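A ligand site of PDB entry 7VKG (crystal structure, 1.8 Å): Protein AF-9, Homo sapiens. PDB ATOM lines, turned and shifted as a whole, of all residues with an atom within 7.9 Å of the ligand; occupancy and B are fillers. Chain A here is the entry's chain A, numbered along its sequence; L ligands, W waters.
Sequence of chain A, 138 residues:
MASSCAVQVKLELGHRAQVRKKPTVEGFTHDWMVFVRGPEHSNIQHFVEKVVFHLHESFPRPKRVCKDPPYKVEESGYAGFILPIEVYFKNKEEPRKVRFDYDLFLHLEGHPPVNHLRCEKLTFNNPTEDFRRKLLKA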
ATOM      1  N   THR A  24     -26.096  29.100  -1.768  1.00  0.00           N
ATOM      2  CA  THR A  24     -25.514  28.458  -0.597  1.00  0.00           C
ATOM      3  C   THR A  24     -24.779  29.501   0.251  1.00  0.00           C
ATOM      4  O   THR A  24     -24.627  30.658  -0.137  1.00  0.00           O
ATOM      5  CB  THR A  24     -24.565  27.353  -1.017  1.00  0.00           C
ATOM      6  OG1 THR A  24     -23.418  27.925  -1.637  1.00  0.00           O
ATOM      7  CG2 THR A  24     -25.236  26.405  -1.996  1.00  0.00           C
ATOM      8  N   GLU A  26     -21.696  29.588   0.681  1.00  0.00           N
ATOM      9  CA  GLU A  26     -20.550  29.989  -0.122  1.00  0.00           C
ATOM     10  C   GLU A  26     -20.929  30.913  -1.263  1.00  0.00           C
ATOM     11  O   GLU A  26     -20.043  31.424  -1.962  1.00  0.00           O
ATOM     12  CB  GLU A  26     -19.834  28.753  -0.677  1.00  0.00           C
ATOM     13  CG  GLU A  26     -19.437  27.709   0.375  1.00  0.00           C
ATOM     14  CD  GLU A  26     -20.468  26.600   0.534  1.00  0.00           C
ATOM     15  OE1 GLU A  26     -21.608  26.758   0.035  1.00  0.00           O
ATOM     16  OE2 GLU A  26     -20.144  25.575   1.171  1.00  0.00           O
ATOM     17  N   PHE A  28     -22.788  29.823  -3.803  1.00  0.00           N
ATOM     18  CA  PHE A  28     -22.988  28.998  -4.982  1.00  0.00           C
ATOM     19  C   PHE A  28     -24.412  29.176  -5.497  1.00  0.00           C
ATOM     20  O   PHE A  28     -25.372  29.081  -4.724  1.00  0.00           O
ATOM     21  CB  PHE A  28     -22.719  27.527  -4.678  1.00  0.00           C
ATOM     22  CG  PHE A  28     -21.325  27.255  -4.184  1.00  0.00           C
ATOM     23  CD1 PHE A  28     -20.267  28.091  -4.535  1.00  0.00           C
ATOM     24  CD2 PHE A  28     -21.068  26.156  -3.385  1.00  0.00           C
ATOM     25  CE1 PHE A  28     -18.985  27.829  -4.086  1.00  0.00           C
ATOM     26  CE2 PHE A  28     -19.783  25.896  -2.926  1.00  0.00           C
ATOM     27  CZ  PHE A  28     -18.737  26.734  -3.284  1.00  0.00           C
ATOM     28  N   THR A  29     -24.540  29.412  -6.798  1.00  0.00           N
ATOM     29  CA  THR A  29     -25.821  29.752  -7.407  1.00  0.00           C
ATOM     30  C   THR A  29     -26.526  28.565  -8.044  1.00  0.00           C
ATOM     31  O   THR A  29     -27.748  28.624  -8.245  1.00  0.00           O
ATOM     32  CB  THR A  29     -25.620  30.827  -8.479  1.00  0.00           C
ATOM     33  OG1 THR A  29     -24.663  30.373  -9.442  1.00  0.00           O
ATOM     34  CG2 THR A  29     -25.099  32.111  -7.839  1.00  0.00           C
ATOM     35  N   HIS A  30     -25.812  27.488  -8.339  1.00  0.00           N
ATOM     36  CA  HIS A  30     -26.329  26.383  -9.131  1.00  0.00           C
ATOM     37  C   HIS A  30     -26.181  25.069  -8.384  1.00  0.00           C
ATOM     38  O   HIS A  30     -25.194  24.864  -7.672  1.00  0.00           O
ATOM     39  CB  HIS A  30     -25.592  26.269 -10.482  1.00  0.00           C
ATOM     40  CG  HIS A  30     -25.972  27.310 -11.476  1.00  0.00           C
ATOM     41  ND1 HIS A  30     -25.584  28.629 -11.359  1.00  0.00           N
ATOM     42  CD2 HIS A  30     -26.681  27.229 -12.631  1.00  0.00           C
ATOM     43  CE1 HIS A  30     -26.056  29.318 -12.395  1.00  0.00           C
ATOM     44  NE2 HIS A  30     -26.711  28.493 -13.180  1.00  0.00           N
ATOM     45  N   TRP A  32     -25.923  21.035  -9.538  1.00  0.00           N
ATOM     46  CA  TRP A  32     -25.726  20.242 -10.748  1.00  0.00           C
ATOM     47  C   TRP A  32     -25.427  18.790 -10.415  1.00  0.00           C
ATOM     48  O   TRP A  32     -25.075  18.431  -9.279  1.00  0.00           O
ATOM     49  CB  TRP A  32     -24.620  20.842 -11.657  1.00  0.00           C
ATOM     50  CG  TRP A  32     -23.256  21.040 -11.068  1.00  0.00           C
ATOM     51  CD1 TRP A  32     -22.696  22.239 -10.690  1.00  0.00           C
ATOM     52  CD2 TRP A  32     -22.228  20.051 -10.856  1.00  0.00           C
ATOM     53  NE1 TRP A  32     -21.415  22.045 -10.237  1.00  0.00           N
ATOM     54  CE2 TRP A  32     -21.107  20.711 -10.319  1.00  0.00           C
ATOM     55  CE3 TRP A  32     -22.172  18.676 -11.054  1.00  0.00           C
ATOM     56  CZ2 TRP A  32     -19.932  20.040  -9.985  1.00  0.00           C
ATOM     57  CZ3 TRP A  32     -20.998  17.997 -10.708  1.00  0.00           C
ATOM     58  CH2 TRP A  32     -19.894  18.681 -10.189  1.00  0.00           C
ATOM     59  N   LEU A  55     -13.147  16.650 -10.673  1.00  0.00           N
ATOM     60  CA  LEU A  55     -13.754  17.967 -10.522  1.00  0.00           C
ATOM     61  C   LEU A  55     -12.682  19.052 -10.586  1.00  0.00           C
ATOM     62  O   LEU A  55     -11.480  18.790 -10.505  1.00  0.00           O
ATOM     63  CB  LEU A  55     -14.532  18.067  -9.207  1.00  0.00           C
ATOM     64  CG  LEU A  55     -15.564  16.970  -8.920  1.00  0.00           C
ATOM     65  CD1 LEU A  55     -16.460  17.346  -7.744  1.00  0.00           C
ATOM     66  CD2 LEU A  55     -16.396  16.662 -10.153  1.00  0.00           C
ATOM     67  N   HIS A  56     -13.136  20.290 -10.750  1.00  0.00           N
ATOM     68  CA  HIS A  56     -12.233  21.436 -10.674  1.00  0.00           C
ATOM     69  C   HIS A  56     -11.479  21.424  -9.342  1.00  0.00           C
ATOM     70  O   HIS A  56     -12.001  20.977  -8.313  1.00  0.00           O
ATOM     71  CB  HIS A  56     -13.012  22.739 -10.833  1.00  0.00           C
ATOM     72  CG  HIS A  56     -12.134  23.949 -11.013  1.00  0.00           C
ATOM     73  ND1 HIS A  56     -11.718  24.730  -9.963  1.00  0.00           N
ATOM     74  CD2 HIS A  56     -11.594  24.496 -12.136  1.00  0.00           C
ATOM     75  CE1 HIS A  56     -10.955  25.712 -10.416  1.00  0.00           C
ATOM     76  NE2 HIS A  56     -10.868  25.590 -11.731  1.00  0.00           N
ATOM     77  N   GLU A  57     -10.249  21.918  -9.383  1.00  0.00           N
ATOM     78  CA  GLU A  57      -9.376  21.871  -8.208  1.00  0.00           C
ATOM     79  C   GLU A  57      -9.975  22.602  -7.003  1.00  0.00           C
ATOM     80  O   GLU A  57      -9.626  22.280  -5.859  1.00  0.00           O
ATOM     81  CB  GLU A  57      -8.015  22.474  -8.557  1.00  0.00           C
ATOM     82  CG  GLU A  57      -8.012  23.985  -8.718  1.00  0.00           C
ATOM     83  CD  GLU A  57      -6.744  24.498  -9.376  1.00  0.00           C
ATOM     84  OE1 GLU A  57      -5.763  24.775  -8.656  1.00  0.00           O
ATOM     85  OE2 GLU A  57      -6.738  24.640 -10.618  1.00  0.00           O
ATOM     86  N   SER A  58     -10.881  23.563  -7.224  1.00  0.00           N
ATOM     87  CA  SER A  58     -11.505  24.286  -6.126  1.00  0.00           C
ATOM     88  C   SER A  58     -12.455  23.421  -5.308  1.00  0.00           C
ATOM     89  O   SER A  58     -12.861  23.835  -4.210  1.00  0.00           O
ATOM     90  CB  SER A  58     -12.258  25.500  -6.660  1.00  0.00           C
ATOM     91  OG  SER A  58     -13.290  25.109  -7.552  1.00  0.00           O
ATOM     92  N   PHE A  59     -12.846  22.245  -5.805  1.00  0.00           N
ATOM     93  CA  PHE A  59     -13.783  21.395  -5.078  1.00  0.00           C
ATOM     94  C   PHE A  59     -13.052  20.563  -4.025  1.00  0.00           C
ATOM     95  O   PHE A  59     -11.922  20.136  -4.251  1.00  0.00           O
ATOM     96  CB  PHE A  59     -14.536  20.476  -6.031  1.00  0.00           C
ATOM     97  CG  PHE A  59     -15.648  21.156  -6.775  1.00  0.00           C
ATOM     98  CD1 PHE A  59     -15.407  21.856  -7.946  1.00  0.00           C
ATOM     99  CD2 PHE A  59     -16.956  21.086  -6.306  1.00  0.00           C
ATOM    100  CE1 PHE A  59     -16.433  22.484  -8.630  1.00  0.00           C
ATOM    101  CE2 PHE A  59     -17.992  21.711  -6.976  1.00  0.00           C
ATOM    102  CZ  PHE A  59     -17.726  22.412  -8.145  1.00  0.00           C
ATOM    103  N   PRO A  60     -13.671  20.333  -2.868  1.00  0.00           N
ATOM    104  CA  PRO A  60     -13.101  19.373  -1.912  1.00  0.00           C
ATOM    105  C   PRO A  60     -13.118  17.978  -2.499  1.00  0.00           C
ATOM    106  O   PRO A  60     -14.091  17.558  -3.119  1.00  0.00           O
ATOM    107  CB  PRO A  60     -14.030  19.485  -0.692  1.00  0.00           C
ATOM    108  CG  PRO A  60     -15.288  20.105  -1.215  1.00  0.00           C
ATOM    109  CD  PRO A  60     -14.866  21.001  -2.336  1.00  0.00           C
ATOM    110  N   ARG A  64     -13.487  12.195  -7.587  1.00  0.00           N
ATOM    111  CA  ARG A  64     -14.661  11.486  -7.102  1.00  0.00           C
ATOM    112  C   ARG A  64     -14.768  10.150  -7.813  1.00  0.00           C
ATOM    113  O   ARG A  64     -14.773  10.098  -9.049  1.00  0.00           O
ATOM    114  CB  ARG A  64     -15.928  12.324  -7.325  1.00  0.00           C
ATOM    115  CG  ARG A  64     -15.832  13.727  -6.757  1.00  0.00           C
ATOM    116  CD  ARG A  64     -15.985  13.728  -5.242  1.00  0.00           C
ATOM    117  NE  ARG A  64     -15.852  15.094  -4.716  1.00  0.00           N
ATOM    118  CZ  ARG A  64     -16.869  15.912  -4.514  1.00  0.00           C
ATOM    119  NH1 ARG A  64     -18.116  15.539  -4.750  1.00  0.00           N
ATOM    120  NH2 ARG A  64     -16.627  17.146  -4.066  1.00  0.00           N
ATOM    121  N   GLU A  75     -23.364  18.107  -6.975  1.00  0.00           N
ATOM    122  CA  GLU A  75     -22.623  19.172  -6.325  1.00  0.00           C
ATOM    123  C   GLU A  75     -23.359  20.492  -6.524  1.00  0.00           C
ATOM    124  O   GLU A  75     -24.358  20.579  -7.239  1.00  0.00           O
ATOM    125  CB  GLU A  75     -21.190  19.291  -6.879  1.00  0.00           C
ATOM    126  CG  GLU A  75     -20.154  18.475  -6.132  1.00  0.00           C
ATOM    127  CD  GLU A  75     -19.989  18.918  -4.692  1.00  0.00           C
ATOM    128  OE1 GLU A  75     -20.301  20.095  -4.375  1.00  0.00           O
ATOM    129  OE2 GLU A  75     -19.544  18.094  -3.866  1.00  0.00           O
ATOM    130  N   SER A  76     -22.847  21.530  -5.862  1.00  0.00           N
ATOM    131  CA  SER A  76     -23.244  22.904  -6.095  1.00  0.00           C
ATOM    132  C   SER A  76     -22.026  23.718  -6.492  1.00  0.00           C
ATOM    133  O   SER A  76     -20.893  23.372  -6.128  1.00  0.00           O
ATOM    134  CB  SER A  76     -23.918  23.507  -4.857  1.00  0.00           C
ATOM    135  OG  SER A  76     -25.192  22.963  -4.655  1.00  0.00           O
ATOM    136  N   GLY A  77     -22.256  24.789  -7.233  1.00  0.00           N
ATOM    137  CA  GLY A  77     -21.143  25.595  -7.697  1.00  0.00           C
ATOM    138  C   GLY A  77     -21.627  26.891  -8.308  1.00  0.00           C
ATOM    139  O   GLY A  77     -22.822  27.177  -8.331  1.00  0.00           O
ATOM    140  N   TYR A  78     -20.675  27.674  -8.807  1.00  0.00           N
ATOM    141  CA  TYR A  78     -20.981  28.977  -9.376  1.00  0.00           C
ATOM    142  C   TYR A  78     -20.525  29.150 -10.820  1.00  0.00           C
ATOM    143  O   TYR A  78     -20.859  30.178 -11.421  1.00  0.00           O
ATOM    144  CB  TYR A  78     -20.363  30.104  -8.517  1.00  0.00           C
ATOM    145  CG  TYR A  78     -18.855  30.143  -8.552  1.00  0.00           C
ATOM    146  CD1 TYR A  78     -18.184  30.866  -9.530  1.00  0.00           C
ATOM    147  CD2 TYR A  78     -18.101  29.473  -7.602  1.00  0.00           C
ATOM    148  CE1 TYR A  78     -16.799  30.911  -9.563  1.00  0.00           C
ATOM    149  CE2 TYR A  78     -16.716  29.511  -7.623  1.00  0.00           C
ATOM    150  CZ  TYR A  78     -16.073  30.231  -8.612  1.00  0.00           C
ATOM    151  OH  TYR A  78     -14.697  30.280  -8.642  1.00  0.00           O
ATOM    152  N   ALA A  79     -19.771  28.208 -11.381  1.00  0.00           N
ATOM    153  CA  ALA A  79     -19.283  28.369 -12.739  1.00  0.00           C
ATOM    154  C   ALA A  79     -19.082  26.998 -13.367  1.00  0.00           C
ATOM    155  O   ALA A  79     -18.830  26.005 -12.675  1.00  0.00           O
ATOM    156  CB  ALA A  79     -17.975  29.165 -12.781  1.00  0.00           C
ATOM    157  N   GLY A  80     -19.192  26.953 -14.693  1.00  0.00           N
ATOM    158  CA  GLY A  80     -18.942  25.715 -15.409  1.00  0.00           C
ATOM    159  C   GLY A  80     -17.462  25.460 -15.634  1.00  0.00           C
ATOM    160  O   GLY A  80     -16.615  26.348 -15.485  1.00  0.00           O
ATOM    161  N   PHE A  81     -17.138  24.229 -16.013  1.00  0.00           N
ATOM    162  CA  PHE A  81     -15.750  23.832 -16.198  1.00  0.00           C
ATOM    163  C   PHE A  81     -15.706  22.540 -17.013  1.00  0.00           C
ATOM    164  O   PHE A  81     -16.710  21.849 -17.161  1.00  0.00           O
ATOM    165  CB  PHE A  81     -15.021  23.652 -14.868  1.00  0.00           C
ATOM    166  CG  PHE A  81     -15.691  22.672 -13.935  1.00  0.00           C
ATOM    167  CD1 PHE A  81     -16.753  23.060 -13.129  1.00  0.00           C
ATOM    168  CD2 PHE A  81     -15.243  21.358 -13.856  1.00  0.00           C
ATOM    169  CE1 PHE A  81     -17.359  22.167 -12.273  1.00  0.00           C
ATOM    170  CE2 PHE A  81     -15.853  20.456 -12.997  1.00  0.00           C
ATOM    171  CZ  PHE A  81     -16.914  20.852 -12.203  1.00  0.00           C
ATOM    172  N   ILE A  82     -14.521  22.239 -17.521  1.00  0.00           N
ATOM    173  CA  ILE A  82     -14.299  20.959 -18.189  1.00  0.00           C
ATOM    174  C   ILE A  82     -14.003  19.900 -17.141  1.00  0.00           C
ATOM    175  O   ILE A  82     -13.131  20.080 -16.283  1.00  0.00           O
ATOM    176  CB  ILE A  82     -13.144  21.058 -19.195  1.00  0.00           C
ATOM    177  CG1 ILE A  82     -13.461  22.095 -20.275  1.00  0.00           C
ATOM    178  CG2 ILE A  82     -12.869  19.692 -19.818  1.00  0.00           C
ATOM    179  CD1 ILE A  82     -12.277  22.428 -21.149  1.00  0.00           C
ATOM    180  N   LEU A 104     -19.017  20.607 -18.413  1.00  0.00           N
ATOM    181  CA  LEU A 104     -20.027  20.821 -17.391  1.00  0.00           C
ATOM    182  C   LEU A 104     -20.404  22.298 -17.419  1.00  0.00           C
ATOM    183  O   LEU A 104     -19.855  23.106 -16.689  1.00  0.00           O
ATOM    184  CB  LEU A 104     -19.497  20.398 -16.023  1.00  0.00           C
ATOM    185  CG  LEU A 104     -20.394  20.166 -14.796  1.00  0.00           C
ATOM    186  CD1 LEU A 104     -21.073  21.449 -14.303  1.00  0.00           C
ATOM    187  CD2 LEU A 104     -21.429  19.087 -15.068  1.00  0.00           C
ATOM    188  N   LEU A 106     -23.116  25.626 -17.195  1.00  0.00           N
ATOM    189  CA  LEU A 106     -24.264  26.119 -16.456  1.00  0.00           C
ATOM    190  C   LEU A 106     -24.901  27.262 -17.249  1.00  0.00           C
ATOM    191  O   LEU A 106     -24.216  27.999 -17.944  1.00  0.00           O
ATOM    192  CB  LEU A 106     -23.874  26.617 -15.051  1.00  0.00           C
ATOM    193  CG  LEU A 106     -22.918  25.754 -14.227  1.00  0.00           C
ATOM    194  CD1 LEU A 106     -22.590  26.435 -12.896  1.00  0.00           C
ATOM    195  CD2 LEU A 106     -23.475  24.363 -13.994  1.00  0.00           C
HETATM  196  C1  LIG L   1     -15.262  26.545  -9.830  1.00  0.00           C
HETATM  197  C2  LIG L   1     -16.182  24.543  -3.897  1.00  0.00           C
HETATM  198  C3  LIG L   1     -15.399  26.352 -12.201  1.00  0.00           C
HETATM  199  C4  LIG L   1     -15.898  26.053 -10.962  1.00  0.00           C
HETATM  200  C5  LIG L   1     -17.545  25.811  -6.593  1.00  0.00           C
HETATM  201  C6  LIG L   1     -17.181  26.125  -8.106  1.00  0.00           C
HETATM  202  C7  LIG L   1     -15.752  25.001  -5.312  1.00  0.00           C
HETATM  203  C8  LIG L   1     -14.264  27.129 -12.327  1.00  0.00           C
HETATM  204  C9  LIG L   1     -13.638  27.610 -11.210  1.00  0.00           C
HETATM  205  C10 LIG L   1     -17.188  23.610  -3.747  1.00  0.00           C
HETATM  206  C11 LIG L   1     -15.545  25.073  -2.748  1.00  0.00           C
HETATM  207  C12 LIG L   1     -17.589  23.180  -2.432  1.00  0.00           C
HETATM  208  C13 LIG L   1     -15.951  24.656  -1.433  1.00  0.00           C
HETATM  209  C14 LIG L   1     -16.964  23.714  -1.289  1.00  0.00           C
HETATM  210  C15 LIG L   1     -14.131  27.313  -9.953  1.00  0.00           C
HETATM  211  N1  LIG L   1     -15.753  26.254  -8.466  1.00  0.00           N
HETATM  212  O1  LIG L   1     -18.050  26.264  -8.929  1.00  0.00           O
HETATM  213  O2  LIG L   1     -16.734  24.697  -6.179  1.00  0.00           O
HETATM  214 CL1  LIG L   1     -13.588  27.528 -14.007  1.00  0.00          CL
HETATM  215  O   HOH W   1     -15.825  28.766 -16.013  1.00  0.00           O
HETATM  216  O   HOH W   2     -17.516  25.311   1.725  1.00  0.00           O
HETATM  217  O   HOH W   3     -19.592  24.346 -10.564  1.00  0.00           O
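OG of Ser 58 sits at hydrogen-bond distance from N1 of the ligand (2.9 Å).
The backbone NH of Tyr 78 sits at hydrogen-bond distance from an oxygen (O1) of the ligand (3.0 Å).
ND1 of His 56 is in hydrogen-bond range of OG of Ser 58, at 2.9 Å.
The backbone NH of Gly 77 lies within hydrogen-bond range of the backbone carbonyl oxygen of His 30.
O of Gly 77 lies within hydrogen-bond range of N of Thr 29 (3.2 Å).
The side-chain hydroxyl (OG1) of Thr 24 lies within hydrogen-bond range of the backbone NH (N) of Phe 28 (2.9 Å).
The guanidinium group (NH2) of Arg 64 sits at hydrogen-bond distance from the backbone carbonyl oxygen (O) of Pro 60 (2.7 Å).
The backbone carbonyl oxygen (O) of Phe 81 lies within hydrogen-bond range of the backbone NH (N) of Leu 104, 2.9 Å away.
Phe 28 touches the ligand.
CE1 of His 56 touches C9 of the ligand, at 3.4 Å.
Phe 59 touches the ligand (CZ to O2, 3.2 Å).
Pro 60 touches the ligand.
Gly 77 touches the ligand (CA to O1, 3.4 Å).
Ala 79 touches the ligand.
Gly 80 touches the ligand (O to C3, 3.5 Å).
Phe 81 touches the ligand.
Hydrophobic or aromatic side chains that line the ligand: Phe 28, His 56, Phe 59, Pro 60, Tyr 78, Ala 79 and Phe 81.
Of the 23 residues printed, 10 come within 4 Å of the ligand.
Water W3 lies within hydrogen-bond range of the backbone carbonyl oxygen (O) of Ala 79 (2.8 Å), the indole nitrogen (NE1) of Trp 32 (3.0 Å) and an oxygen (O1) of the ligand (3.0 Å).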
